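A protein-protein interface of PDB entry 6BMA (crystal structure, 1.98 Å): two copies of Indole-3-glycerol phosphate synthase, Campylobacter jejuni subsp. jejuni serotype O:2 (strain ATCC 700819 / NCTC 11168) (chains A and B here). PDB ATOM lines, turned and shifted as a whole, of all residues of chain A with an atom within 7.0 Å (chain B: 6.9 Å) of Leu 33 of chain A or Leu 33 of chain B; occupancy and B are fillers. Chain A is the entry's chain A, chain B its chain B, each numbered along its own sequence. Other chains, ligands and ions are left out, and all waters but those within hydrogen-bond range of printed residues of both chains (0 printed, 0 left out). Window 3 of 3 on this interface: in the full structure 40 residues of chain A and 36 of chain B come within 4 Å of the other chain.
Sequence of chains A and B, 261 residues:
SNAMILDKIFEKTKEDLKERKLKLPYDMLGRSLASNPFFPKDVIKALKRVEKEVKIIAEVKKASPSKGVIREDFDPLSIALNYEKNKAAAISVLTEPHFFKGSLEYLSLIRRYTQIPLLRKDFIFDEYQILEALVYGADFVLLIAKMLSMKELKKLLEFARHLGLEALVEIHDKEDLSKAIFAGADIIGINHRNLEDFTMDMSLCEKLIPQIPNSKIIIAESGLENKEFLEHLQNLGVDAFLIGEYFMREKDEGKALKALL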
ATOM      1  N   MET A  28      -5.209   9.887 -27.408  1.00  0.00           N
ATOM      2  CA  MET A  28      -6.538  10.488 -27.398  1.00  0.00           C
ATOM      3  C   MET A  28      -6.765  11.375 -26.181  1.00  0.00           C
ATOM      4  O   MET A  28      -7.520  12.348 -26.262  1.00  0.00           O
ATOM      5  CB  MET A  28      -7.622   9.402 -27.440  1.00  0.00           C
ATOM      6  CG  MET A  28      -7.595   8.514 -28.683  1.00  0.00           C
ATOM      7  SD  MET A  28      -7.799   9.383 -30.275  1.00  0.00           S
ATOM      8  CE  MET A  28      -9.530   9.804 -30.204  1.00  0.00           C
ATOM      9  N   LEU A  29      -6.115  11.064 -25.060  1.00  0.00           N
ATOM     10  CA  LEU A  29      -6.298  11.846 -23.843  1.00  0.00           C
ATOM     11  C   LEU A  29      -5.861  13.294 -24.061  1.00  0.00           C
ATOM     12  O   LEU A  29      -6.616  14.234 -23.803  1.00  0.00           O
ATOM     13  CB  LEU A  29      -5.505  11.207 -22.699  1.00  0.00           C
ATOM     14  CG  LEU A  29      -5.520  11.918 -21.345  1.00  0.00           C
ATOM     15  CD1 LEU A  29      -6.940  12.048 -20.854  1.00  0.00           C
ATOM     16  CD2 LEU A  29      -4.687  11.163 -20.310  1.00  0.00           C
ATOM     17  N   GLY A  30      -4.633  13.482 -24.532  1.00  0.00           N
ATOM     18  CA  GLY A  30      -4.110  14.826 -24.705  1.00  0.00           C
ATOM     19  C   GLY A  30      -4.669  15.539 -25.923  1.00  0.00           C
ATOM     20  O   GLY A  30      -5.071  16.707 -25.845  1.00  0.00           O
ATOM     21  N   ARG A  31      -4.707  14.855 -27.070  1.00  0.00           N
ATOM     22  CA  ARG A  31      -5.100  15.537 -28.302  1.00  0.00           C
ATOM     23  C   ARG A  31      -6.588  15.885 -28.352  1.00  0.00           C
ATOM     24  O   ARG A  31      -6.971  16.807 -29.081  1.00  0.00           O
ATOM     25  CB  ARG A  31      -4.734  14.690 -29.524  1.00  0.00           C
ATOM     26  CG  ARG A  31      -3.228  14.652 -29.824  1.00  0.00           C
ATOM     27  CD  ARG A  31      -2.976  13.963 -31.155  1.00  0.00           C
ATOM     28  NE  ARG A  31      -3.481  12.593 -31.146  1.00  0.00           N
ATOM     29  CZ  ARG A  31      -3.699  11.873 -32.238  1.00  0.00           C
ATOM     30  NH1 ARG A  31      -4.156  10.629 -32.125  1.00  0.00           N
ATOM     31  NH2 ARG A  31      -3.475  12.416 -33.442  1.00  0.00           N
ATOM     32  N   SER A  32      -7.440  15.182 -27.605  1.00  0.00           N
ATOM     33  CA  SER A  32      -8.873  15.403 -27.776  1.00  0.00           C
ATOM     34  C   SER A  32      -9.291  16.802 -27.343  1.00  0.00           C
ATOM     35  O   SER A  32     -10.376  17.258 -27.723  1.00  0.00           O
ATOM     36  CB  SER A  32      -9.680  14.343 -27.013  1.00  0.00           C
ATOM     37  OG  SER A  32      -9.709  13.102 -27.718  1.00  0.00           O
ATOM     38  N   LEU A  33      -8.447  17.493 -26.584  1.00  0.00           N
ATOM     39  CA  LEU A  33      -8.700  18.848 -26.143  1.00  0.00           C
ATOM     40  C   LEU A  33      -7.981  19.899 -27.000  1.00  0.00           C
ATOM     41  O   LEU A  33      -8.119  21.097 -26.734  1.00  0.00           O
ATOM     42  CB  LEU A  33      -8.304  18.990 -24.667  1.00  0.00           C
ATOM     43  CG  LEU A  33      -9.230  18.392 -23.582  1.00  0.00           C
ATOM     44  CD1 LEU A  33     -10.558  19.122 -23.560  1.00  0.00           C
ATOM     45  CD2 LEU A  33      -9.454  16.893 -23.740  1.00  0.00           C
ATOM     46  N   ALA A  34      -7.214  19.488 -28.013  1.00  0.00           N
ATOM     47  CA  ALA A  34      -6.876  20.389 -29.109  1.00  0.00           C
ATOM     48  C   ALA A  34      -8.130  20.630 -29.949  1.00  0.00           C
ATOM     49  O   ALA A  34      -9.214  20.149 -29.631  1.00  0.00           O
ATOM     50  CB  ALA A  34      -5.747  19.812 -29.956  1.00  0.00           C
ATOM     51  N   SER A  35      -8.009  21.363 -31.052  1.00  0.00           N
ATOM     52  CA  SER A  35      -9.258  21.748 -31.710  1.00  0.00           C
ATOM     53  C   SER A  35      -9.545  20.975 -32.993  1.00  0.00           C
ATOM     54  O   SER A  35      -9.919  21.586 -34.000  1.00  0.00           O
ATOM     55  CB  SER A  35      -9.266  23.246 -32.021  1.00  0.00           C
ATOM     56  OG  SER A  35      -9.529  24.003 -30.857  1.00  0.00           O
ATOM     57  N   ASN A  36      -9.380  19.651 -32.980  1.00  0.00           N
ATOM     58  CA  ASN A  36      -9.811  18.857 -34.122  1.00  0.00           C
ATOM     59  C   ASN A  36     -11.304  19.072 -34.351  1.00  0.00           C
ATOM     60  O   ASN A  36     -12.084  19.063 -33.390  1.00  0.00           O
ATOM     61  CB  ASN A  36      -9.550  17.370 -33.901  1.00  0.00           C
ATOM     62  CG  ASN A  36      -8.092  17.024 -33.949  1.00  0.00           C
ATOM     63  OD1 ASN A  36      -7.545  16.764 -35.018  1.00  0.00           O
ATOM     64  ND2 ASN A  36      -7.446  17.018 -32.785  1.00  0.00           N
ATOM     65  N   PRO A  40      -9.159  13.048 -33.167  1.00  0.00           N
ATOM     66  CA  PRO A  40      -7.759  12.982 -33.604  1.00  0.00           C
ATOM     67  C   PRO A  40      -7.511  11.745 -34.453  1.00  0.00           C
ATOM     68  O   PRO A  40      -8.142  10.703 -34.266  1.00  0.00           O
ATOM     69  CB  PRO A  40      -6.973  12.923 -32.288  1.00  0.00           C
ATOM     70  CG  PRO A  40      -7.912  13.460 -31.242  1.00  0.00           C
ATOM     71  CD  PRO A  40      -9.282  13.046 -31.696  1.00  0.00           C
ATOM     72  N   LEU A 134       1.018  20.272 -28.928  1.00  0.00           N
ATOM     73  CA  LEU A 134      -0.226  19.623 -28.511  1.00  0.00           C
ATOM     74  C   LEU A 134      -1.381  20.610 -28.520  1.00  0.00           C
ATOM     75  O   LEU A 134      -2.426  20.369 -29.137  1.00  0.00           O
ATOM     76  CB  LEU A 134      -0.073  19.015 -27.109  1.00  0.00           C
ATOM     77  CG  LEU A 134      -1.329  18.382 -26.495  1.00  0.00           C
ATOM     78  CD1 LEU A 134      -1.781  17.189 -27.321  1.00  0.00           C
ATOM     79  CD2 LEU A 134      -1.073  17.942 -25.036  1.00  0.00           C
ATOM     80  N   VAL A 135      -1.206  21.733 -27.817  1.00  0.00           N
ATOM     81  CA  VAL A 135      -2.287  22.693 -27.603  1.00  0.00           C
ATOM     82  C   VAL A 135      -2.715  23.330 -28.915  1.00  0.00           C
ATOM     83  O   VAL A 135      -3.907  23.583 -29.133  1.00  0.00           O
ATOM     84  CB  VAL A 135      -1.833  23.746 -26.568  1.00  0.00           C
ATOM     85  CG1 VAL A 135      -2.769  24.919 -26.537  1.00  0.00           C
ATOM     86  CG2 VAL A 135      -1.756  23.106 -25.179  1.00  0.00           C
ATOM     87  N   MET B  28       0.255  28.440 -17.653  1.00  0.00           N
ATOM     88  CA  MET B  28      -0.903  28.953 -18.371  1.00  0.00           C
ATOM     89  C   MET B  28      -1.139  28.239 -19.689  1.00  0.00           C
ATOM     90  O   MET B  28      -2.297  28.088 -20.106  1.00  0.00           O
ATOM     91  CB  MET B  28      -0.749  30.460 -18.622  1.00  0.00           C
ATOM     92  CG  MET B  28      -0.614  31.256 -17.314  1.00  0.00           C
ATOM     93  SD  MET B  28      -2.052  31.025 -16.212  1.00  0.00           S
ATOM     94  CE  MET B  28      -3.183  32.183 -16.968  1.00  0.00           C
ATOM     95  N   LEU B  29      -0.073  27.771 -20.338  1.00  0.00           N
ATOM     96  CA  LEU B  29      -0.216  27.137 -21.643  1.00  0.00           C
ATOM     97  C   LEU B  29      -1.000  25.834 -21.528  1.00  0.00           C
ATOM     98  O   LEU B  29      -1.951  25.596 -22.286  1.00  0.00           O
ATOM     99  CB  LEU B  29       1.175  26.898 -22.260  1.00  0.00           C
ATOM    100  CG  LEU B  29       1.271  26.015 -23.505  1.00  0.00           C
ATOM    101  CD1 LEU B  29       0.507  26.622 -24.685  1.00  0.00           C
ATOM    102  CD2 LEU B  29       2.737  25.754 -23.879  1.00  0.00           C
ATOM    103  N   GLY B  30      -0.627  24.986 -20.574  1.00  0.00           N
ATOM    104  CA  GLY B  30      -1.280  23.699 -20.419  1.00  0.00           C
ATOM    105  C   GLY B  30      -2.654  23.778 -19.790  1.00  0.00           C
ATOM    106  O   GLY B  30      -3.604  23.174 -20.294  1.00  0.00           O
ATOM    107  N   ARG B  31      -2.786  24.531 -18.691  1.00  0.00           N
ATOM    108  CA  ARG B  31      -4.058  24.523 -17.966  1.00  0.00           C
ATOM    109  C   ARG B  31      -5.171  25.235 -18.727  1.00  0.00           C
ATOM    110  O   ARG B  31      -6.344  25.121 -18.349  1.00  0.00           O
ATOM    111  CB  ARG B  31      -3.869  25.134 -16.577  1.00  0.00           C
ATOM    112  CG  ARG B  31      -3.050  24.233 -15.641  1.00  0.00           C
ATOM    113  CD  ARG B  31      -3.085  24.784 -14.215  1.00  0.00           C
ATOM    114  NE  ARG B  31      -2.376  26.056 -14.149  1.00  0.00           N
ATOM    115  CZ  ARG B  31      -2.481  26.914 -13.139  1.00  0.00           C
ATOM    116  NH1 ARG B  31      -3.276  26.632 -12.116  1.00  0.00           N
ATOM    117  NH2 ARG B  31      -1.802  28.061 -13.168  1.00  0.00           N
ATOM    118  N   SER B  32      -4.834  25.943 -19.807  1.00  0.00           N
ATOM    119  CA  SER B  32      -5.847  26.389 -20.760  1.00  0.00           C
ATOM    120  C   SER B  32      -6.623  25.227 -21.371  1.00  0.00           C
ATOM    121  O   SER B  32      -7.741  25.429 -21.847  1.00  0.00           O
ATOM    122  CB  SER B  32      -5.193  27.183 -21.889  1.00  0.00           C
ATOM    123  OG  SER B  32      -4.488  26.303 -22.760  1.00  0.00           O
ATOM    124  N   LEU B  33      -6.041  24.023 -21.407  1.00  0.00           N
ATOM    125  CA  LEU B  33      -6.783  22.870 -21.911  1.00  0.00           C
ATOM    126  C   LEU B  33      -7.943  22.502 -20.991  1.00  0.00           C
ATOM    127  O   LEU B  33      -8.956  21.969 -21.458  1.00  0.00           O
ATOM    128  CB  LEU B  33      -5.842  21.672 -22.091  1.00  0.00           C
ATOM    129  N   ALA B  34      -7.816  22.779 -19.695  1.00  0.00           N
ATOM    130  CA  ALA B  34      -8.830  22.427 -18.715  1.00  0.00           C
ATOM    131  C   ALA B  34      -9.995  23.411 -18.782  1.00  0.00           C
ATOM    132  O   ALA B  34      -9.945  24.427 -19.476  1.00  0.00           O
ATOM    133  CB  ALA B  34      -8.230  22.413 -17.312  1.00  0.00           C
ATOM    134  N   SER B  35     -11.044  23.104 -18.030  1.00  0.00           N
ATOM    135  CA  SER B  35     -12.300  23.858 -18.085  1.00  0.00           C
ATOM    136  C   SER B  35     -12.450  24.820 -16.910  1.00  0.00           C
ATOM    137  O   SER B  35     -13.509  24.865 -16.284  1.00  0.00           O
ATOM    138  CB  SER B  35     -13.483  22.898 -18.142  1.00  0.00           C
ATOM    139  OG  SER B  35     -13.338  21.989 -19.221  1.00  0.00           O
ATOM    140  N   ASN B  36     -11.409  25.586 -16.582  1.00  0.00           N
ATOM    141  CA  ASN B  36     -11.572  26.649 -15.599  1.00  0.00           C
ATOM    142  C   ASN B  36     -12.698  27.576 -16.049  1.00  0.00           C
ATOM    143  O   ASN B  36     -12.795  27.904 -17.243  1.00  0.00           O
ATOM    144  CB  ASN B  36     -10.287  27.468 -15.438  1.00  0.00           C
ATOM    145  CG  ASN B  36      -9.220  26.753 -14.637  1.00  0.00           C
ATOM    146  OD1 ASN B  36      -9.270  26.714 -13.407  1.00  0.00           O
ATOM    147  ND2 ASN B  36      -8.222  26.224 -15.331  1.00  0.00           N
ATOM    148  N   LEU B 134      -4.101  17.132 -15.621  1.00  0.00           N
ATOM    149  CA  LEU B 134      -4.166  18.351 -16.434  1.00  0.00           C
ATOM    150  C   LEU B 134      -5.517  18.497 -17.133  1.00  0.00           C
ATOM    151  O   LEU B 134      -6.197  19.527 -17.004  1.00  0.00           O
ATOM    152  CB  LEU B 134      -3.047  18.356 -17.489  1.00  0.00           C
ATOM    153  CG  LEU B 134      -3.094  19.541 -18.451  1.00  0.00           C
ATOM    154  CD1 LEU B 134      -2.934  20.834 -17.689  1.00  0.00           C
ATOM    155  CD2 LEU B 134      -2.026  19.423 -19.550  1.00  0.00           C
ATOM    156  N   VAL B 135      -5.896  17.465 -17.895  1.00  0.00           N
ATOM    157  CA  VAL B 135      -7.109  17.494 -18.710  1.00  0.00           C
ATOM    158  C   VAL B 135      -8.336  17.671 -17.828  1.00  0.00           C
ATOM    159  O   VAL B 135      -9.232  18.474 -18.121  1.00  0.00           O
ATOM    160  CB  VAL B 135      -7.203  16.205 -19.554  1.00  0.00           C
ATOM    161  CG1 VAL B 135      -8.530  16.125 -20.289  1.00  0.00           C
ATOM    162  CG2 VAL B 135      -6.036  16.117 -20.532  1.00  0.00           C
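O of Leu 29 of chain B sits at hydrogen-bond distance from OG of Ser 32 of chain B, at 2.7 Å.
O of Leu 29 of chain A touches CG2 of Val 135 of chain B, at 3.8 Å.
Leu 33 of chain A touches Leu 33 of chain B (CD1 to O, 3.9 Å).
Val 135 of chain B touches Leu 33 of chain A.
Val 135 of chain A touches Leu 29 of chain B (CG2 to O, 3.8 Å).
Of the printed residues of chain B, Leu 33 of chain A touches Leu 33 and Val 135.
Pro 40 of chain A touches none of the printed residues of chain B.
Of the printed residues of chain B, Val 135 of chain A touches Leu 29.
Of the printed residues of chain A, Leu 29 of chain B touches Val 135 (3.8 Å).
Ala 34 of chain B touches none of the printed residues of chain A.
The nearest printed residue of chain B that does not touch Leu 33 of chain A is Ser 35 of chain B (5.9 Å).
The nearest printed residue of chain B that does not touch Leu 29 of chain A is Leu 134 of chain B (7.6 Å).
Printed residues of chain A that touch a printed residue of chain B: Leu 29, Leu 33 and Val 135.
Along chain A the printed residues that touch a printed residue of chain B span positions 29 to 135.
Hydrophobic or aromatic side chains of chain B that line the printed part of chain A: Val 135.
Along chain B the printed residues that touch a printed residue of chain A span positions 29 to 135.
Among the printed residues, 4 pairs touch across the chains.
Leu 29 of chain A touches Val 135 of chain B, and with the chains exchanged Val 135 of chain A touches Leu 29 of chain B.
Leu 33 of chain B touches its own counterpart, Leu 33 of chain A.
Leu 33 of chain A touches Val 135 of chain B, but with the chains exchanged Val 135 of chain A does not touch Leu 33 of chain B (5.3 Å).
11 positions are printed for both chains.
Of the 4 pairs that touch across the chains among the printed residues, 3 have their exchanged pair printed and touching as well.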
